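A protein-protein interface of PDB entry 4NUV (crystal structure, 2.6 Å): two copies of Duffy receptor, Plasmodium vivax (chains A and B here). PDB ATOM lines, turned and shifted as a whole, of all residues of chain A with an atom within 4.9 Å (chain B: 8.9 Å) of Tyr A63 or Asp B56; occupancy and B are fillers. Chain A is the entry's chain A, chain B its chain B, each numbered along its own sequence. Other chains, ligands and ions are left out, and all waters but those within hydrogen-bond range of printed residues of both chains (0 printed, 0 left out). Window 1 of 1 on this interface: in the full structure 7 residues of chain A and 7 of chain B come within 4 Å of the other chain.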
ATOM      1  N   ASN A  44      28.558 -32.244 -10.583  1.00  0.00           N
ATOM      2  CA  ASN A  44      27.970 -32.454  -9.265  1.00  0.00           C
ATOM      3  C   ASN A  44      27.314 -31.185  -8.729  1.00  0.00           C
ATOM      4  O   ASN A  44      27.025 -31.079  -7.537  1.00  0.00           O
ATOM      5  CB  ASN A  44      29.030 -32.948  -8.279  1.00  0.00           C
ATOM      6  CG  ASN A  44      29.508 -34.354  -8.590  1.00  0.00           C
ATOM      7  OD1 ASN A  44      30.673 -34.565  -8.931  1.00  0.00           O
ATOM      8  ND2 ASN A  44      28.612 -35.327  -8.462  1.00  0.00           N
ATOM      9  N   LEU A  45      27.080 -30.223  -9.617  1.00  0.00           N
ATOM     10  CA  LEU A  45      26.454 -28.962  -9.241  1.00  0.00           C
ATOM     11  C   LEU A  45      25.148 -29.205  -8.490  1.00  0.00           C
ATOM     12  O   LEU A  45      24.942 -28.673  -7.399  1.00  0.00           O
ATOM     13  CB  LEU A  45      26.188 -28.122 -10.492  1.00  0.00           C
ATOM     14  CG  LEU A  45      25.652 -26.706 -10.284  1.00  0.00           C
ATOM     15  CD1 LEU A  45      26.616 -25.873  -9.462  1.00  0.00           C
ATOM     16  CD2 LEU A  45      25.398 -26.047 -11.629  1.00  0.00           C
ATOM     17  N   THR A  58      22.298 -15.856  -5.459  1.00  0.00           N
ATOM     18  CA  THR A  58      23.650 -16.257  -5.091  1.00  0.00           C
ATOM     19  C   THR A  58      24.024 -17.588  -5.729  1.00  0.00           C
ATOM     20  O   THR A  58      25.201 -17.876  -5.937  1.00  0.00           O
ATOM     21  CB  THR A  58      23.810 -16.395  -3.561  1.00  0.00           C
ATOM     22  OG1 THR A  58      22.985 -17.465  -3.079  1.00  0.00           O
ATOM     23  CG2 THR A  58      23.436 -15.099  -2.855  1.00  0.00           C
ATOM     24  N   PHE A  59      23.018 -18.399  -6.036  1.00  0.00           N
ATOM     25  CA  PHE A  59      23.251 -19.726  -6.588  1.00  0.00           C
ATOM     26  C   PHE A  59      23.903 -19.644  -7.966  1.00  0.00           C
ATOM     27  O   PHE A  59      24.790 -20.434  -8.288  1.00  0.00           O
ATOM     28  CB  PHE A  59      21.937 -20.502  -6.679  1.00  0.00           C
ATOM     29  CG  PHE A  59      22.114 -21.992  -6.691  1.00  0.00           C
ATOM     30  CD1 PHE A  59      22.260 -22.679  -7.884  1.00  0.00           C
ATOM     31  CD2 PHE A  59      22.133 -22.707  -5.505  1.00  0.00           C
ATOM     32  CE1 PHE A  59      22.423 -24.052  -7.891  1.00  0.00           C
ATOM     33  CE2 PHE A  59      22.294 -24.078  -5.508  1.00  0.00           C
ATOM     34  CZ  PHE A  59      22.440 -24.751  -6.703  1.00  0.00           C
ATOM     35  N   LYS A  61      25.059 -16.513  -9.281  1.00  0.00           N
ATOM     36  CA  LYS A  61      26.027 -15.421  -9.288  1.00  0.00           C
ATOM     37  C   LYS A  61      27.319 -15.788  -8.557  1.00  0.00           C
ATOM     38  O   LYS A  61      28.397 -15.314  -8.918  1.00  0.00           O
ATOM     39  CB  LYS A  61      25.420 -14.166  -8.659  1.00  0.00           C
ATOM     40  CG  LYS A  61      24.221 -13.605  -9.411  1.00  0.00           C
ATOM     41  CD  LYS A  61      24.604 -13.102 -10.794  1.00  0.00           C
ATOM     42  CE  LYS A  61      23.402 -12.523 -11.523  1.00  0.00           C
ATOM     43  NZ  LYS A  61      23.749 -12.029 -12.883  1.00  0.00           N
ATOM     44  N   LEU A  62      27.209 -16.627  -7.532  1.00  0.00           N
ATOM     45  CA  LEU A  62      28.372 -17.004  -6.731  1.00  0.00           C
ATOM     46  C   LEU A  62      28.671 -18.496  -6.805  1.00  0.00           C
ATOM     47  O   LEU A  62      29.718 -18.899  -7.306  1.00  0.00           O
ATOM     48  CB  LEU A  62      28.176 -16.580  -5.274  1.00  0.00           C
ATOM     49  CG  LEU A  62      28.463 -15.107  -4.973  1.00  0.00           C
ATOM     50  CD1 LEU A  62      28.013 -14.751  -3.567  1.00  0.00           C
ATOM     51  CD2 LEU A  62      29.945 -14.798  -5.150  1.00  0.00           C
ATOM     52  N   TYR A  63      27.755 -19.315  -6.300  1.00  0.00           N
ATOM     53  CA  TYR A  63      27.974 -20.755  -6.250  1.00  0.00           C
ATOM     54  C   TYR A  63      28.381 -21.298  -7.615  1.00  0.00           C
ATOM     55  O   TYR A  63      29.441 -21.905  -7.761  1.00  0.00           O
ATOM     56  CB  TYR A  63      26.715 -21.467  -5.757  1.00  0.00           C
ATOM     57  CG  TYR A  63      26.888 -22.956  -5.562  1.00  0.00           C
ATOM     58  CD1 TYR A  63      27.803 -23.454  -4.643  1.00  0.00           C
ATOM     59  CD2 TYR A  63      26.126 -23.863  -6.287  1.00  0.00           C
ATOM     60  CE1 TYR A  63      27.961 -24.813  -4.458  1.00  0.00           C
ATOM     61  CE2 TYR A  63      26.276 -25.225  -6.107  1.00  0.00           C
ATOM     62  CZ  TYR A  63      27.194 -25.694  -5.191  1.00  0.00           C
ATOM     63  OH  TYR A  63      27.347 -27.050  -5.010  1.00  0.00           O
ATOM     64  N   LEU A  64      27.532 -21.077  -8.614  1.00  0.00           N
ATOM     65  CA  LEU A  64      27.817 -21.525  -9.970  1.00  0.00           C
ATOM     66  C   LEU A  64      29.175 -21.004 -10.424  1.00  0.00           C
ATOM     67  O   LEU A  64      30.005 -21.759 -10.929  1.00  0.00           O
ATOM     68  CB  LEU A  64      26.729 -21.034 -10.929  1.00  0.00           C
ATOM     69  CG  LEU A  64      26.956 -21.336 -12.414  1.00  0.00           C
ATOM     70  CD1 LEU A  64      26.946 -22.836 -12.674  1.00  0.00           C
ATOM     71  CD2 LEU A  64      25.913 -20.633 -13.269  1.00  0.00           C
ATOM     72  N   LYS A  65      29.390 -19.708 -10.233  1.00  0.00           N
ATOM     73  CA  LYS A  65      30.611 -19.051 -10.676  1.00  0.00           C
ATOM     74  C   LYS A  65      31.847 -19.659 -10.018  1.00  0.00           C
ATOM     75  O   LYS A  65      32.891 -19.803 -10.652  1.00  0.00           O
ATOM     76  CB  LYS A  65      30.535 -17.557 -10.363  1.00  0.00           C
ATOM     77  CG  LYS A  65      31.473 -16.700 -11.190  1.00  0.00           C
ATOM     78  CD  LYS A  65      31.178 -15.222 -10.998  1.00  0.00           C
ATOM     79  CE  LYS A  65      31.429 -14.434 -12.272  1.00  0.00           C
ATOM     80  NZ  LYS A  65      30.197 -13.746 -12.742  1.00  0.00           N
ATOM     81  N   ARG A  66      31.719 -20.015  -8.745  1.00  0.00           N
ATOM     82  CA  ARG A  66      32.838 -20.561  -7.986  1.00  0.00           C
ATOM     83  C   ARG A  66      33.252 -21.935  -8.504  1.00  0.00           C
ATOM     84  O   ARG A  66      34.442 -22.214  -8.664  1.00  0.00           O
ATOM     85  CB  ARG A  66      32.478 -20.646  -6.501  1.00  0.00           C
ATOM     86  CG  ARG A  66      32.431 -19.295  -5.804  1.00  0.00           C
ATOM     87  CD  ARG A  66      31.723 -19.367  -4.460  1.00  0.00           C
ATOM     88  NE  ARG A  66      32.468 -20.153  -3.481  1.00  0.00           N
ATOM     89  CZ  ARG A  66      33.499 -19.699  -2.774  1.00  0.00           C
ATOM     90  NH1 ARG A  66      33.933 -18.454  -2.933  1.00  0.00           N
ATOM     91  NH2 ARG A  66      34.106 -20.494  -1.906  1.00  0.00           N
ATOM     92  N   LYS A  67      32.268 -22.790  -8.767  1.00  0.00           N
ATOM     93  CA  LYS A  67      32.542 -24.148  -9.223  1.00  0.00           C
ATOM     94  C   LYS A  67      33.107 -24.159 -10.643  1.00  0.00           C
ATOM     95  O   LYS A  67      33.898 -25.034 -10.997  1.00  0.00           O
ATOM     96  CB  LYS A  67      31.275 -25.001  -9.144  1.00  0.00           C
ATOM     97  CG  LYS A  67      30.736 -25.150  -7.726  1.00  0.00           C
ATOM     98  CD  LYS A  67      29.592 -26.146  -7.649  1.00  0.00           C
ATOM     99  CE  LYS A  67      30.060 -27.579  -7.839  1.00  0.00           C
ATOM    100  NZ  LYS A  67      30.926 -28.051  -6.722  1.00  0.00           N
ATOM    101  N   HIS B  54      29.441 -29.135   2.522  1.00  0.00           N
ATOM    102  CA  HIS B  54      30.822 -29.523   2.269  1.00  0.00           C
ATOM    103  C   HIS B  54      31.746 -28.308   2.386  1.00  0.00           C
ATOM    104  O   HIS B  54      31.532 -27.445   3.238  1.00  0.00           O
ATOM    105  CB  HIS B  54      30.936 -30.182   0.890  1.00  0.00           C
ATOM    106  CG  HIS B  54      30.515 -29.295  -0.239  1.00  0.00           C
ATOM    107  ND1 HIS B  54      29.200 -28.937  -0.448  1.00  0.00           N
ATOM    108  CD2 HIS B  54      31.226 -28.700  -1.225  1.00  0.00           C
ATOM    109  CE1 HIS B  54      29.121 -28.156  -1.509  1.00  0.00           C
ATOM    110  NE2 HIS B  54      30.338 -27.996  -2.001  1.00  0.00           N
ATOM    111  N   ARG B  55      32.767 -28.240   1.536  1.00  0.00           N
ATOM    112  CA  ARG B  55      33.741 -27.155   1.589  1.00  0.00           C
ATOM    113  C   ARG B  55      33.073 -25.795   1.403  1.00  0.00           C
ATOM    114  O   ARG B  55      33.210 -24.902   2.239  1.00  0.00           O
ATOM    115  CB  ARG B  55      34.789 -27.334   0.492  1.00  0.00           C
ATOM    116  CG  ARG B  55      35.476 -28.688   0.472  1.00  0.00           C
ATOM    117  CD  ARG B  55      35.486 -29.260  -0.937  1.00  0.00           C
ATOM    118  NE  ARG B  55      35.898 -28.265  -1.924  1.00  0.00           N
ATOM    119  CZ  ARG B  55      35.757 -28.404  -3.239  1.00  0.00           C
ATOM    120  NH1 ARG B  55      35.209 -29.499  -3.747  1.00  0.00           N
ATOM    121  NH2 ARG B  55      36.164 -27.438  -4.051  1.00  0.00           N
ATOM    122  N   ASP B  56      32.354 -25.654   0.295  1.00  0.00           N
ATOM    123  CA  ASP B  56      31.785 -24.372  -0.108  1.00  0.00           C
ATOM    124  C   ASP B  56      31.028 -23.688   1.027  1.00  0.00           C
ATOM    125  O   ASP B  56      30.122 -24.266   1.627  1.00  0.00           O
ATOM    126  CB  ASP B  56      30.862 -24.563  -1.313  1.00  0.00           C
ATOM    127  CG  ASP B  56      30.430 -23.248  -1.929  1.00  0.00           C
ATOM    128  OD1 ASP B  56      31.199 -22.686  -2.738  1.00  0.00           O
ATOM    129  OD2 ASP B  56      29.320 -22.773  -1.608  1.00  0.00           O
ATOM    130  N   ILE B  57      31.413 -22.447   1.307  1.00  0.00           N
ATOM    131  CA  ILE B  57      30.782 -21.655   2.356  1.00  0.00           C
ATOM    132  C   ILE B  57      29.407 -21.176   1.905  1.00  0.00           C
ATOM    133  O   ILE B  57      28.414 -21.356   2.611  1.00  0.00           O
ATOM    134  CB  ILE B  57      31.637 -20.425   2.716  1.00  0.00           C
ATOM    135  CG1 ILE B  57      33.041 -20.857   3.149  1.00  0.00           C
ATOM    136  CG2 ILE B  57      30.969 -19.619   3.819  1.00  0.00           C
ATOM    137  CD1 ILE B  57      34.015 -19.708   3.309  1.00  0.00           C
ATOM    138  N   THR B  58      29.357 -20.567   0.725  1.00  0.00           N
ATOM    139  CA  THR B  58      28.114 -20.016   0.197  1.00  0.00           C
ATOM    140  C   THR B  58      27.025 -21.083   0.107  1.00  0.00           C
ATOM    141  O   THR B  58      25.835 -20.772   0.170  1.00  0.00           O
ATOM    142  CB  THR B  58      28.315 -19.391  -1.203  1.00  0.00           C
ATOM    143  OG1 THR B  58      28.710 -20.405  -2.137  1.00  0.00           O
ATOM    144  CG2 THR B  58      29.372 -18.293  -1.162  1.00  0.00           C
ATOM    145  N   PHE B  59      27.434 -22.339  -0.038  1.00  0.00           N
ATOM    146  CA  PHE B  59      26.488 -23.443  -0.143  1.00  0.00           C
ATOM    147  C   PHE B  59      25.799 -23.710   1.190  1.00  0.00           C
ATOM    148  O   PHE B  59      24.573 -23.784   1.261  1.00  0.00           O
ATOM    149  CB  PHE B  59      27.195 -24.710  -0.623  1.00  0.00           C
ATOM    150  CG  PHE B  59      26.331 -25.936  -0.583  1.00  0.00           C
ATOM    151  CD1 PHE B  59      25.375 -26.157  -1.562  1.00  0.00           C
ATOM    152  CD2 PHE B  59      26.473 -26.866   0.432  1.00  0.00           C
ATOM    153  CE1 PHE B  59      24.578 -27.284  -1.527  1.00  0.00           C
ATOM    154  CE2 PHE B  59      25.679 -27.996   0.471  1.00  0.00           C
ATOM    155  CZ  PHE B  59      24.729 -28.204  -0.510  1.00  0.00           C
ATOM    156  N   ARG B  60      26.592 -23.860   2.245  1.00  0.00           N
ATOM    157  CA  ARG B  60      26.051 -24.104   3.576  1.00  0.00           C
ATOM    158  C   ARG B  60      25.186 -22.931   4.022  1.00  0.00           C
ATOM    159  O   ARG B  60      24.158 -23.116   4.672  1.00  0.00           O
ATOM    160  CB  ARG B  60      27.179 -24.344   4.581  1.00  0.00           C
ATOM    161  CG  ARG B  60      27.993 -25.594   4.299  1.00  0.00           C
ATOM    162  CD  ARG B  60      28.665 -26.120   5.556  1.00  0.00           C
ATOM    163  NE  ARG B  60      29.171 -27.478   5.377  1.00  0.00           N
ATOM    164  CZ  ARG B  60      28.405 -28.565   5.342  1.00  0.00           C
ATOM    165  NH1 ARG B  60      27.088 -28.463   5.464  1.00  0.00           N
ATOM    166  NH2 ARG B  60      28.955 -29.760   5.175  1.00  0.00           N
ATOM    167  N   LYS B  61      25.609 -21.724   3.663  1.00  0.00           N
ATOM    168  CA  LYS B  61      24.844 -20.522   3.965  1.00  0.00           C
ATOM    169  C   LYS B  61      23.437 -20.637   3.391  1.00  0.00           C
ATOM    170  O   LYS B  61      22.466 -20.196   4.006  1.00  0.00           O
ATOM    171  CB  LYS B  61      25.541 -19.291   3.386  1.00  0.00           C
ATOM    172  CG  LYS B  61      26.930 -19.041   3.951  1.00  0.00           C
ATOM    173  CD  LYS B  61      26.954 -17.852   4.899  1.00  0.00           C
ATOM    174  CE  LYS B  61      27.783 -16.703   4.339  1.00  0.00           C
ATOM    175  NZ  LYS B  61      27.282 -16.200   3.026  1.00  0.00           N
ATOM    176  N   LEU B  62      23.334 -21.232   2.206  1.00  0.00           N
ATOM    177  CA  LEU B  62      22.045 -21.397   1.545  1.00  0.00           C
ATOM    178  C   LEU B  62      21.261 -22.550   2.156  1.00  0.00           C
ATOM    179  O   LEU B  62      20.044 -22.468   2.310  1.00  0.00           O
ATOM    180  CB  LEU B  62      22.230 -21.630   0.045  1.00  0.00           C
ATOM    181  CG  LEU B  62      21.609 -20.555  -0.847  1.00  0.00           C
ATOM    182  CD1 LEU B  62      22.256 -19.202  -0.590  1.00  0.00           C
ATOM    183  CD2 LEU B  62      21.729 -20.940  -2.312  1.00  0.00           C
ATOM    184  N   TYR B  63      21.959 -23.626   2.503  1.00  0.00           N
ATOM    185  CA  TYR B  63      21.320 -24.756   3.163  1.00  0.00           C
ATOM    186  C   TYR B  63      20.796 -24.314   4.527  1.00  0.00           C
ATOM    187  O   TYR B  63      19.843 -24.887   5.057  1.00  0.00           O
ATOM    188  CB  TYR B  63      22.302 -25.918   3.317  1.00  0.00           C
ATOM    189  CG  TYR B  63      21.687 -27.159   3.923  1.00  0.00           C
ATOM    190  CD1 TYR B  63      20.593 -27.775   3.329  1.00  0.00           C
ATOM    191  CD2 TYR B  63      22.204 -27.719   5.084  1.00  0.00           C
ATOM    192  CE1 TYR B  63      20.026 -28.910   3.879  1.00  0.00           C
ATOM    193  CE2 TYR B  63      21.645 -28.857   5.640  1.00  0.00           C
ATOM    194  CZ  TYR B  63      20.555 -29.447   5.033  1.00  0.00           C
ATOM    195  OH  TYR B  63      19.995 -30.578   5.580  1.00  0.00           O
ATOM    196  N   SER B 126      29.949 -24.374  13.119  1.00  0.00           N
ATOM    197  CA  SER B 126      30.367 -25.340  12.113  1.00  0.00           C
ATOM    198  C   SER B 126      30.136 -24.822  10.695  1.00  0.00           C
ATOM    199  O   SER B 126      30.636 -25.398   9.729  1.00  0.00           O
ATOM    200  CB  SER B 126      29.609 -26.653  12.306  1.00  0.00           C
ATOM    201  OG  SER B 126      29.888 -27.562  11.257  1.00  0.00           O
ATOM    202  N   ILE B 127      29.377 -23.739  10.570  1.00  0.00           N
ATOM    203  CA  ILE B 127      29.046 -23.184   9.263  1.00  0.00           C
ATOM    204  C   ILE B 127      29.794 -21.884   8.977  1.00  0.00           C
ATOM    205  O   ILE B 127      30.278 -21.671   7.865  1.00  0.00           O
ATOM    206  CB  ILE B 127      27.529 -22.940   9.138  1.00  0.00           C
ATOM    207  CG1 ILE B 127      26.808 -24.265   8.883  1.00  0.00           C
ATOM    208  CG2 ILE B 127      27.233 -21.959   8.012  1.00  0.00           C
ATOM    209  CD1 ILE B 127      25.300 -24.164   8.893  1.00  0.00           C
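NE of Arg A66 is in salt-bridge range of OD1 of Asp B56 (2.9 Å).
Of the 11 printed residues of chain A, 4 touch a printed residue of chain B.
Printed residues of chain A that touch a printed residue of chain B: Thr A58, Phe A59, Tyr A63 and Arg A66.
Hydrophobic or aromatic side chains of chain B within 4 Å of the printed part of chain A: Phe B59 and Leu B62.
Among the printed residues, 6 pairs touch across the chains.
OG1 of Thr B58 is in hydrogen-bond range of OD2 of Asp B56 (2.5 Å).
N of Phe B59 lies within hydrogen-bond range of OD2 of Asp B56 (2.5 Å).
O of Thr A58 is in hydrogen-bond range of N of Tyr A63, 3.0 Å away.
The backbone NH (N) of Leu A64 is in hydrogen-bond range of the backbone carbonyl oxygen (O) of Phe A59 (2.8 Å).
OG1 of Thr A58 touches CD1 of Leu B62, 3.1 Å away.
Leu B62 touches Phe A59 (CD2 to CD2, 3.7 Å).
Asp B56 touches Tyr A63 (OD2 to CD1, 3.5 Å).
CB of Phe B59 touches CE1 of Tyr A63 (3.9 Å).
Thr B58 touches Arg A66 (OG1 to CD, 3.9 Å).
Printed residues of chain B within 4 Å of Thr A58: Leu B62 (3.1 Å).
Of the printed residues of chain B, Phe A59 touches Leu B62 (3.7 Å).
Printed residues of chain B within 4 Å of Tyr A63: Asp B56 and Phe B59.
Leu A64 touches none of the printed residues of chain B.
Printed residues of chain B within 4 Å of Arg A66: Asp B56 and Thr B58.
Printed residues of chain A within 4 Å of Thr B58: Arg A66.
The nearest printed residue of chain B that does not touch Tyr A63 is Thr B58 (4.05 Å).
Thr A58 touches Leu B62, but with the chains exchanged Leu A62 does not touch Thr B58 (4.5 Å).
Phe A59 touches Leu B62, but with the chains exchanged Leu A62 does not touch Phe B59 (7.8 Å).
Tyr A63 touches Phe B59, but with the chains exchanged Phe A59 does not touch Tyr B63 (8.0 Å).
Positions printed for both chains: 58, 59, 61, 62 and 63.
Of the 6 pairs that touch across the chains among the printed residues, none has its exchanged pair printed and touching as well.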
